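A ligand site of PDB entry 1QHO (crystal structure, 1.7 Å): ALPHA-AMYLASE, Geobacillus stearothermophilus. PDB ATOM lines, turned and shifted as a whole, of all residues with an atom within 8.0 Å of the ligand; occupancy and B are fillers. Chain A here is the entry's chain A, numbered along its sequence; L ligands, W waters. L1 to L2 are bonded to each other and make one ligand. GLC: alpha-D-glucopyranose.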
ATOM      1  N   THR A 603       4.747  17.145  16.034  1.00  0.00           N
ATOM      2  CA  THR A 603       5.864  16.937  16.964  1.00  0.00           C
ATOM      3  C   THR A 603       6.011  15.442  17.195  1.00  0.00           C
ATOM      4  O   THR A 603       5.030  14.696  17.021  1.00  0.00           O
ATOM      5  CB  THR A 603       5.682  17.753  18.245  1.00  0.00           C
ATOM      6  OG1 THR A 603       6.905  17.698  19.013  1.00  0.00           O
ATOM      7  CG2 THR A 603       4.545  17.247  19.107  1.00  0.00           C
ATOM      8  N   GLY A 604       7.215  14.969  17.496  1.00  0.00           N
ATOM      9  CA  GLY A 604       7.385  13.513  17.595  1.00  0.00           C
ATOM     10  C   GLY A 604       8.704  13.120  18.245  1.00  0.00           C
ATOM     11  O   GLY A 604       9.454  13.974  18.727  1.00  0.00           O
ATOM     12  N   ASN A 605       8.999  11.821  18.198  1.00  0.00           N
ATOM     13  CA  ASN A 605      10.086  11.271  19.007  1.00  0.00           C
ATOM     14  C   ASN A 605      11.457  11.237  18.370  1.00  0.00           C
ATOM     15  O   ASN A 605      12.268  10.355  18.689  1.00  0.00           O
ATOM     16  CB  ASN A 605       9.662   9.851  19.440  1.00  0.00           C
ATOM     17  CG  ASN A 605       9.676   8.864  18.284  1.00  0.00           C
ATOM     18  OD1 ASN A 605       9.633   9.217  17.098  1.00  0.00           O
ATOM     19  ND2 ASN A 605       9.754   7.572  18.612  1.00  0.00           N
ATOM     20  N   ASN A 611      11.507  16.232  19.111  1.00  0.00           N
ATOM     21  CA  ASN A 611      11.557  15.490  20.363  1.00  0.00           C
ATOM     22  C   ASN A 611      10.461  15.929  21.330  1.00  0.00           C
ATOM     23  O   ASN A 611      10.676  16.236  22.513  1.00  0.00           O
ATOM     24  CB  ASN A 611      12.915  15.622  21.053  1.00  0.00           C
ATOM     25  CG  ASN A 611      13.973  14.823  20.310  1.00  0.00           C
ATOM     26  OD1 ASN A 611      13.751  13.658  19.962  1.00  0.00           O
ATOM     27  ND2 ASN A 611      15.113  15.464  20.074  1.00  0.00           N
ATOM     28  N   TRP A 612       9.230  15.951  20.840  1.00  0.00           N
ATOM     29  CA  TRP A 612       8.019  16.288  21.566  1.00  0.00           C
ATOM     30  C   TRP A 612       7.881  17.723  22.034  1.00  0.00           C
ATOM     31  O   TRP A 612       6.998  18.061  22.816  1.00  0.00           O
ATOM     32  CB  TRP A 612       7.854  15.299  22.754  1.00  0.00           C
ATOM     33  CG  TRP A 612       7.711  13.874  22.306  1.00  0.00           C
ATOM     34  CD1 TRP A 612       8.611  12.869  22.552  1.00  0.00           C
ATOM     35  CD2 TRP A 612       6.700  13.308  21.488  1.00  0.00           C
ATOM     36  NE1 TRP A 612       8.183  11.695  21.965  1.00  0.00           N
ATOM     37  CE2 TRP A 612       6.989  11.944  21.333  1.00  0.00           C
ATOM     38  CE3 TRP A 612       5.513  13.817  20.929  1.00  0.00           C
ATOM     39  CZ2 TRP A 612       6.183  11.083  20.579  1.00  0.00           C
ATOM     40  CZ3 TRP A 612       4.685  12.963  20.220  1.00  0.00           C
ATOM     41  CH2 TRP A 612       5.037  11.615  20.036  1.00  0.00           C
ATOM     42  N   SER A 613       8.692  18.643  21.502  1.00  0.00           N
ATOM     43  CA  SER A 613       8.585  20.042  21.850  1.00  0.00           C
ATOM     44  C   SER A 613       7.260  20.628  21.353  1.00  0.00           C
ATOM     45  O   SER A 613       6.791  20.238  20.285  1.00  0.00           O
ATOM     46  CB  SER A 613       9.741  20.805  21.175  1.00  0.00           C
ATOM     47  OG  SER A 613       9.646  22.189  21.409  1.00  0.00           O
ATOM     48  N   THR A 614       6.751  21.638  22.067  1.00  0.00           N
ATOM     49  CA  THR A 614       5.620  22.413  21.566  1.00  0.00           C
ATOM     50  C   THR A 614       6.071  23.855  21.302  1.00  0.00           C
ATOM     51  O   THR A 614       5.250  24.739  21.052  1.00  0.00           O
ATOM     52  CB  THR A 614       4.417  22.443  22.522  1.00  0.00           C
ATOM     53  OG1 THR A 614       4.847  22.985  23.791  1.00  0.00           O
ATOM     54  CG2 THR A 614       3.850  21.042  22.733  1.00  0.00           C
ATOM     55  N   GLN A 648       7.242   7.982  15.976  1.00  0.00           N
ATOM     56  CA  GLN A 648       6.013   8.235  16.732  1.00  0.00           C
ATOM     57  C   GLN A 648       5.780   9.754  16.735  1.00  0.00           C
ATOM     58  O   GLN A 648       6.731  10.526  16.824  1.00  0.00           O
ATOM     59  CB  GLN A 648       6.071   7.708  18.168  1.00  0.00           C
ATOM     60  CG  GLN A 648       6.260   6.204  18.213  1.00  0.00           C
ATOM     61  CD  GLN A 648       5.738   5.573  19.484  1.00  0.00           C
ATOM     62  OE1 GLN A 648       5.055   6.206  20.301  1.00  0.00           O
ATOM     63  NE2 GLN A 648       6.066   4.306  19.663  1.00  0.00           N
ATOM     64  N   PHE A 649       4.525  10.151  16.554  1.00  0.00           N
ATOM     65  CA  PHE A 649       4.233  11.569  16.433  1.00  0.00           C
ATOM     66  C   PHE A 649       2.778  11.859  16.794  1.00  0.00           C
ATOM     67  O   PHE A 649       1.891  11.002  16.854  1.00  0.00           O
ATOM     68  CB  PHE A 649       4.523  12.047  15.000  1.00  0.00           C
ATOM     69  CG  PHE A 649       3.744  11.317  13.941  1.00  0.00           C
ATOM     70  CD1 PHE A 649       4.177  10.103  13.450  1.00  0.00           C
ATOM     71  CD2 PHE A 649       2.566  11.856  13.448  1.00  0.00           C
ATOM     72  CE1 PHE A 649       3.432   9.404  12.510  1.00  0.00           C
ATOM     73  CE2 PHE A 649       1.829  11.191  12.480  1.00  0.00           C
ATOM     74  CZ  PHE A 649       2.265   9.956  12.016  1.00  0.00           C
ATOM     75  N   LYS A 650       2.553  13.126  17.121  1.00  0.00           N
ATOM     76  CA  LYS A 650       1.223  13.670  17.317  1.00  0.00           C
ATOM     77  C   LYS A 650       1.194  15.105  16.757  1.00  0.00           C
ATOM     78  O   LYS A 650       2.233  15.728  16.542  1.00  0.00           O
ATOM     79  CB  LYS A 650       0.784  13.741  18.768  1.00  0.00           C
ATOM     80  CG  LYS A 650       0.308  12.431  19.398  1.00  0.00           C
ATOM     81  CD  LYS A 650      -0.355  12.839  20.724  1.00  0.00           C
ATOM     82  CE  LYS A 650      -1.139  11.705  21.346  1.00  0.00           C
ATOM     83  NZ  LYS A 650      -1.858  12.212  22.562  1.00  0.00           N
ATOM     84  N   PHE A 651      -0.022  15.593  16.569  1.00  0.00           N
ATOM     85  CA  PHE A 651      -0.254  16.968  16.135  1.00  0.00           C
ATOM     86  C   PHE A 651      -0.865  17.735  17.311  1.00  0.00           C
ATOM     87  O   PHE A 651      -1.435  17.140  18.235  1.00  0.00           O
ATOM     88  CB  PHE A 651      -1.224  17.028  14.952  1.00  0.00           C
ATOM     89  CG  PHE A 651      -0.683  16.293  13.748  1.00  0.00           C
ATOM     90  CD1 PHE A 651      -0.923  14.942  13.582  1.00  0.00           C
ATOM     91  CD2 PHE A 651       0.070  16.961  12.790  1.00  0.00           C
ATOM     92  CE1 PHE A 651      -0.415  14.266  12.496  1.00  0.00           C
ATOM     93  CE2 PHE A 651       0.569  16.297  11.687  1.00  0.00           C
ATOM     94  CZ  PHE A 651       0.338  14.934  11.538  1.00  0.00           C
ATOM     95  N   PHE A 652      -0.696  19.050  17.285  1.00  0.00           N
ATOM     96  CA  PHE A 652      -1.300  19.881  18.318  1.00  0.00           C
ATOM     97  C   PHE A 652      -1.719  21.201  17.682  1.00  0.00           C
ATOM     98  O   PHE A 652      -1.153  21.640  16.674  1.00  0.00           O
ATOM     99  CB  PHE A 652      -0.388  20.120  19.511  1.00  0.00           C
ATOM    100  CG  PHE A 652       0.862  20.918  19.281  1.00  0.00           C
ATOM    101  CD1 PHE A 652       0.849  22.297  19.296  1.00  0.00           C
ATOM    102  CD2 PHE A 652       2.073  20.267  19.086  1.00  0.00           C
ATOM    103  CE1 PHE A 652       2.016  23.016  19.096  1.00  0.00           C
ATOM    104  CE2 PHE A 652       3.246  20.983  18.899  1.00  0.00           C
ATOM    105  CZ  PHE A 652       3.221  22.368  18.889  1.00  0.00           C
ATOM    106  N   ILE A 660      -1.968  25.493  24.040  1.00  0.00           N
ATOM    107  CA  ILE A 660      -1.699  24.267  23.305  1.00  0.00           C
ATOM    108  C   ILE A 660      -2.800  23.235  23.488  1.00  0.00           C
ATOM    109  O   ILE A 660      -3.152  22.886  24.619  1.00  0.00           O
ATOM    110  CB  ILE A 660      -0.370  23.609  23.760  1.00  0.00           C
ATOM    111  CG1 ILE A 660       0.818  24.541  23.568  1.00  0.00           C
ATOM    112  CG2 ILE A 660      -0.143  22.299  23.027  1.00  0.00           C
ATOM    113  CD1 ILE A 660       1.065  24.972  22.136  1.00  0.00           C
ATOM    114  N   GLN A 661      -3.343  22.703  22.398  1.00  0.00           N
ATOM    115  CA  GLN A 661      -4.345  21.659  22.464  1.00  0.00           C
ATOM    116  C   GLN A 661      -3.831  20.445  21.684  1.00  0.00           C
ATOM    117  O   GLN A 661      -3.810  20.419  20.451  1.00  0.00           O
ATOM    118  CB  GLN A 661      -5.723  22.034  21.919  1.00  0.00           C
ATOM    119  CG  GLN A 661      -6.698  20.855  21.964  1.00  0.00           C
ATOM    120  CD  GLN A 661      -8.071  21.238  21.451  1.00  0.00           C
ATOM    121  OE1 GLN A 661      -8.508  22.381  21.612  1.00  0.00           O
ATOM    122  NE2 GLN A 661      -8.753  20.291  20.833  1.00  0.00           N
ATOM    123  N   TRP A 662      -3.383  19.429  22.417  1.00  0.00           N
ATOM    124  CA  TRP A 662      -2.880  18.220  21.797  1.00  0.00           C
ATOM    125  C   TRP A 662      -3.988  17.346  21.221  1.00  0.00           C
ATOM    126  O   TRP A 662      -5.110  17.333  21.749  1.00  0.00           O
ATOM    127  CB  TRP A 662      -2.190  17.354  22.849  1.00  0.00           C
ATOM    128  CG  TRP A 662      -0.864  17.822  23.351  1.00  0.00           C
ATOM    129  CD1 TRP A 662      -0.624  18.659  24.403  1.00  0.00           C
ATOM    130  CD2 TRP A 662       0.424  17.410  22.868  1.00  0.00           C
ATOM    131  NE1 TRP A 662       0.734  18.810  24.590  1.00  0.00           N
ATOM    132  CE2 TRP A 662       1.397  18.056  23.658  1.00  0.00           C
ATOM    133  CE3 TRP A 662       0.830  16.557  21.838  1.00  0.00           C
ATOM    134  CZ2 TRP A 662       2.754  17.857  23.464  1.00  0.00           C
ATOM    135  CZ3 TRP A 662       2.185  16.366  21.640  1.00  0.00           C
ATOM    136  CH2 TRP A 662       3.126  17.028  22.433  1.00  0.00           C
ATOM    137  N   GLU A 663      -3.629  16.525  20.231  1.00  0.00           N
ATOM    138  CA  GLU A 663      -4.488  15.427  19.859  1.00  0.00           C
ATOM    139  C   GLU A 663      -4.583  14.516  21.103  1.00  0.00           C
ATOM    140  O   GLU A 663      -3.604  14.433  21.849  1.00  0.00           O
ATOM    141  CB  GLU A 663      -3.874  14.476  18.841  1.00  0.00           C
ATOM    142  CG  GLU A 663      -4.192  14.694  17.381  1.00  0.00           C
ATOM    143  CD  GLU A 663      -3.485  13.617  16.570  1.00  0.00           C
ATOM    144  OE1 GLU A 663      -2.237  13.683  16.460  1.00  0.00           O
ATOM    145  OE2 GLU A 663      -4.184  12.725  16.078  1.00  0.00           O
ATOM    146  N   ASN A 664      -5.701  13.826  21.245  1.00  0.00           N
ATOM    147  CA  ASN A 664      -5.801  12.915  22.386  1.00  0.00           C
ATOM    148  C   ASN A 664      -5.305  11.536  21.972  1.00  0.00           C
ATOM    149  O   ASN A 664      -4.811  11.365  20.857  1.00  0.00           O
ATOM    150  CB  ASN A 664      -7.254  12.897  22.875  1.00  0.00           C
ATOM    151  CG  ASN A 664      -7.584  14.152  23.670  1.00  0.00           C
ATOM    152  OD1 ASN A 664      -6.759  14.660  24.446  1.00  0.00           O
ATOM    153  ND2 ASN A 664      -8.795  14.659  23.493  1.00  0.00           N
ATOM    154  N   GLY A 665      -5.413  10.589  22.891  1.00  0.00           N
ATOM    155  CA  GLY A 665      -5.039   9.206  22.657  1.00  0.00           C
ATOM    156  C   GLY A 665      -3.562   8.923  22.546  1.00  0.00           C
ATOM    157  O   GLY A 665      -2.689   9.700  22.933  1.00  0.00           O
ATOM    158  N   SER A 666      -3.249   7.756  21.972  1.00  0.00           N
ATOM    159  CA  SER A 666      -1.884   7.300  21.828  1.00  0.00           C
ATOM    160  C   SER A 666      -1.204   7.925  20.606  1.00  0.00           C
ATOM    161  O   SER A 666      -1.827   8.377  19.650  1.00  0.00           O
ATOM    162  CB  SER A 666      -1.797   5.776  21.686  1.00  0.00           C
ATOM    163  OG  SER A 666      -2.438   5.137  22.780  1.00  0.00           O
ATOM    164  N   ASN A 667       0.123   7.892  20.676  1.00  0.00           N
ATOM    165  CA  ASN A 667       0.899   8.439  19.557  1.00  0.00           C
ATOM    166  C   ASN A 667       0.594   7.691  18.260  1.00  0.00           C
ATOM    167  O   ASN A 667       0.317   6.492  18.254  1.00  0.00           O
ATOM    168  CB  ASN A 667       2.401   8.259  19.796  1.00  0.00           C
ATOM    169  CG  ASN A 667       2.911   9.019  20.988  1.00  0.00           C
ATOM    170  OD1 ASN A 667       2.330  10.020  21.372  1.00  0.00           O
ATOM    171  ND2 ASN A 667       4.038   8.559  21.540  1.00  0.00           N
ATOM    172  N   HIS A 668       0.693   8.444  17.154  1.00  0.00           N
ATOM    173  CA  HIS A 668       0.536   7.857  15.829  1.00  0.00           C
ATOM    174  C   HIS A 668       1.893   7.199  15.544  1.00  0.00           C
ATOM    175  O   HIS A 668       2.932   7.688  16.007  1.00  0.00           O
ATOM    176  CB  HIS A 668       0.302   8.861  14.713  1.00  0.00           C
ATOM    177  CG  HIS A 668      -1.031   9.543  14.798  1.00  0.00           C
ATOM    178  ND1 HIS A 668      -2.168   8.962  14.289  1.00  0.00           N
ATOM    179  CD2 HIS A 668      -1.391  10.750  15.299  1.00  0.00           C
ATOM    180  CE1 HIS A 668      -3.201   9.779  14.491  1.00  0.00           C
ATOM    181  NE2 HIS A 668      -2.746  10.859  15.108  1.00  0.00           N
ATOM    182  N   GLN A 685      -6.998  12.462  16.344  1.00  0.00           N
ATOM    183  CA  GLN A 685      -7.616  11.685  17.435  1.00  0.00           C
ATOM    184  C   GLN A 685      -8.285  12.596  18.454  1.00  0.00           C
ATOM    185  O   GLN A 685      -7.639  13.409  19.107  1.00  0.00           O
ATOM    186  CB  GLN A 685      -6.533  10.815  18.106  1.00  0.00           C
ATOM    187  CG  GLN A 685      -6.006   9.757  17.155  1.00  0.00           C
ATOM    188  CD  GLN A 685      -4.786   9.008  17.634  1.00  0.00           C
ATOM    189  OE1 GLN A 685      -4.335   8.078  16.943  1.00  0.00           O
ATOM    190  NE2 GLN A 685      -4.205   9.377  18.771  1.00  0.00           N
HETATM  191  C1  GLC L   1      -0.620  15.503  26.588  1.00  0.00           C
HETATM  192  C2  GLC L   1      -0.705  14.711  25.284  1.00  0.00           C
HETATM  193  C3  GLC L   1       0.447  13.700  25.180  1.00  0.00           C
HETATM  194  C4  GLC L   1       1.772  14.442  25.351  1.00  0.00           C
HETATM  195  C5  GLC L   1       1.767  15.182  26.695  1.00  0.00           C
HETATM  196  C6  GLC L   1       3.021  16.020  26.884  1.00  0.00           C
HETATM  197  O1  GLC L   1      -0.830  14.602  27.642  1.00  0.00           O
HETATM  198  O2  GLC L   1      -1.914  13.991  25.214  1.00  0.00           O
HETATM  199  O3  GLC L   1       0.437  13.078  23.902  1.00  0.00           O
HETATM  200  O4  GLC L   1       2.814  13.478  25.343  1.00  0.00           O
HETATM  201  O5  GLC L   1       0.657  16.067  26.766  1.00  0.00           O
HETATM  202  O6  GLC L   1       3.124  16.531  28.210  1.00  0.00           O
HETATM  203  C1  GLC L   2       3.771  13.548  24.298  1.00  0.00           C
HETATM  204  C2  GLC L   2       3.898  12.140  23.696  1.00  0.00           C
HETATM  205  C3  GLC L   2       4.554  11.213  24.743  1.00  0.00           C
HETATM  206  C4  GLC L   2       5.891  11.826  25.160  1.00  0.00           C
HETATM  207  C5  GLC L   2       5.659  13.220  25.730  1.00  0.00           C
HETATM  208  C6  GLC L   2       6.957  13.933  26.094  1.00  0.00           C
HETATM  209  O2  GLC L   2       2.620  11.662  23.338  1.00  0.00           O
HETATM  210  O3  GLC L   2       4.770   9.965  24.102  1.00  0.00           O
HETATM  211  O4  GLC L   2       6.512  10.994  26.142  1.00  0.00           O
HETATM  212  O5  GLC L   2       5.021  14.027  24.735  1.00  0.00           O
HETATM  213  O6  GLC L   2       6.646  15.158  26.744  1.00  0.00           O
HETATM  214  O   HOH W   1       4.602  19.296  26.716  1.00  0.00           O
HETATM  215  O   HOH W   2      -1.200  15.257  30.171  1.00  0.00           O
HETATM  216  O   HOH W   3       8.963  10.799  25.771  1.00  0.00           O
HETATM  217  O   HOH W   4      -2.502  11.586  26.634  1.00  0.00           O
HETATM  218  O   HOH W   5       6.092  17.440  25.238  1.00  0.00           O
HETATM  219  O   HOH W   6       1.917   8.828  24.820  1.00  0.00           O
HETATM  220  O   HOH W   7      -4.243  15.321  25.500  1.00  0.00           O
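NZ of Lys 650 lies within hydrogen-bond range of O3 of GLC L1 (2.8 Å). The side-chain amide oxygen of Asn 667 is in hydrogen-bond range of an oxygen (O2) of GLC L2 (2.6 Å).
Water W7 lies within hydrogen-bond range of an oxygen (O2) of GLC L1 and the side-chain amide oxygen (OD1) of Asn 664. Water W5 bridges O of Trp 612 (2.7 Å) and O6 of GLC L2 (2.8 Å).
Residues that only touch the ligand: Trp 662 (3.5 Å), Trp 612 (3.6 Å) and Glu 663 (3.8 Å). Hydrophobic or aromatic side chains within 4 Å of the ligand: Trp 612 and Trp 662. Of the 22 residues printed, 5 come within 4 Å of the ligand. The nearest printed residue that does not touch the ligand is Gly 665 (4.7 Å).
The backbone NH of Phe 651 lies within hydrogen-bond range of the side-chain carboxylate of Glu 663. The backbone NH (N) of Thr 603 lies within hydrogen-bond range of the backbone carbonyl oxygen (O) of Lys 650, at 2.9 Å. The backbone NH (N) of Gln 685 is in hydrogen-bond range of the side-chain carboxylate (OE2) of Glu 663, at 2.8 Å. N of Trp 612 lies close to OG1 of Thr 603 (3.4 Å). The backbone NH (N) of Trp 612 is in hydrogen-bond range of the backbone carbonyl oxygen (O) of Gly 604 (2.9 Å). The side-chain amino group (NZ) of Lys 650 is in hydrogen-bond range of the backbone carbonyl oxygen (O) of Glu 663, at 2.9 Å. ND2 of Asn 667 sits at hydrogen-bond distance from OE1 of Gln 648 (2.8 Å). The side-chain carboxylate (OE2) of Glu 663 is in hydrogen-bond range of a ring nitrogen (NE2) of His 668.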
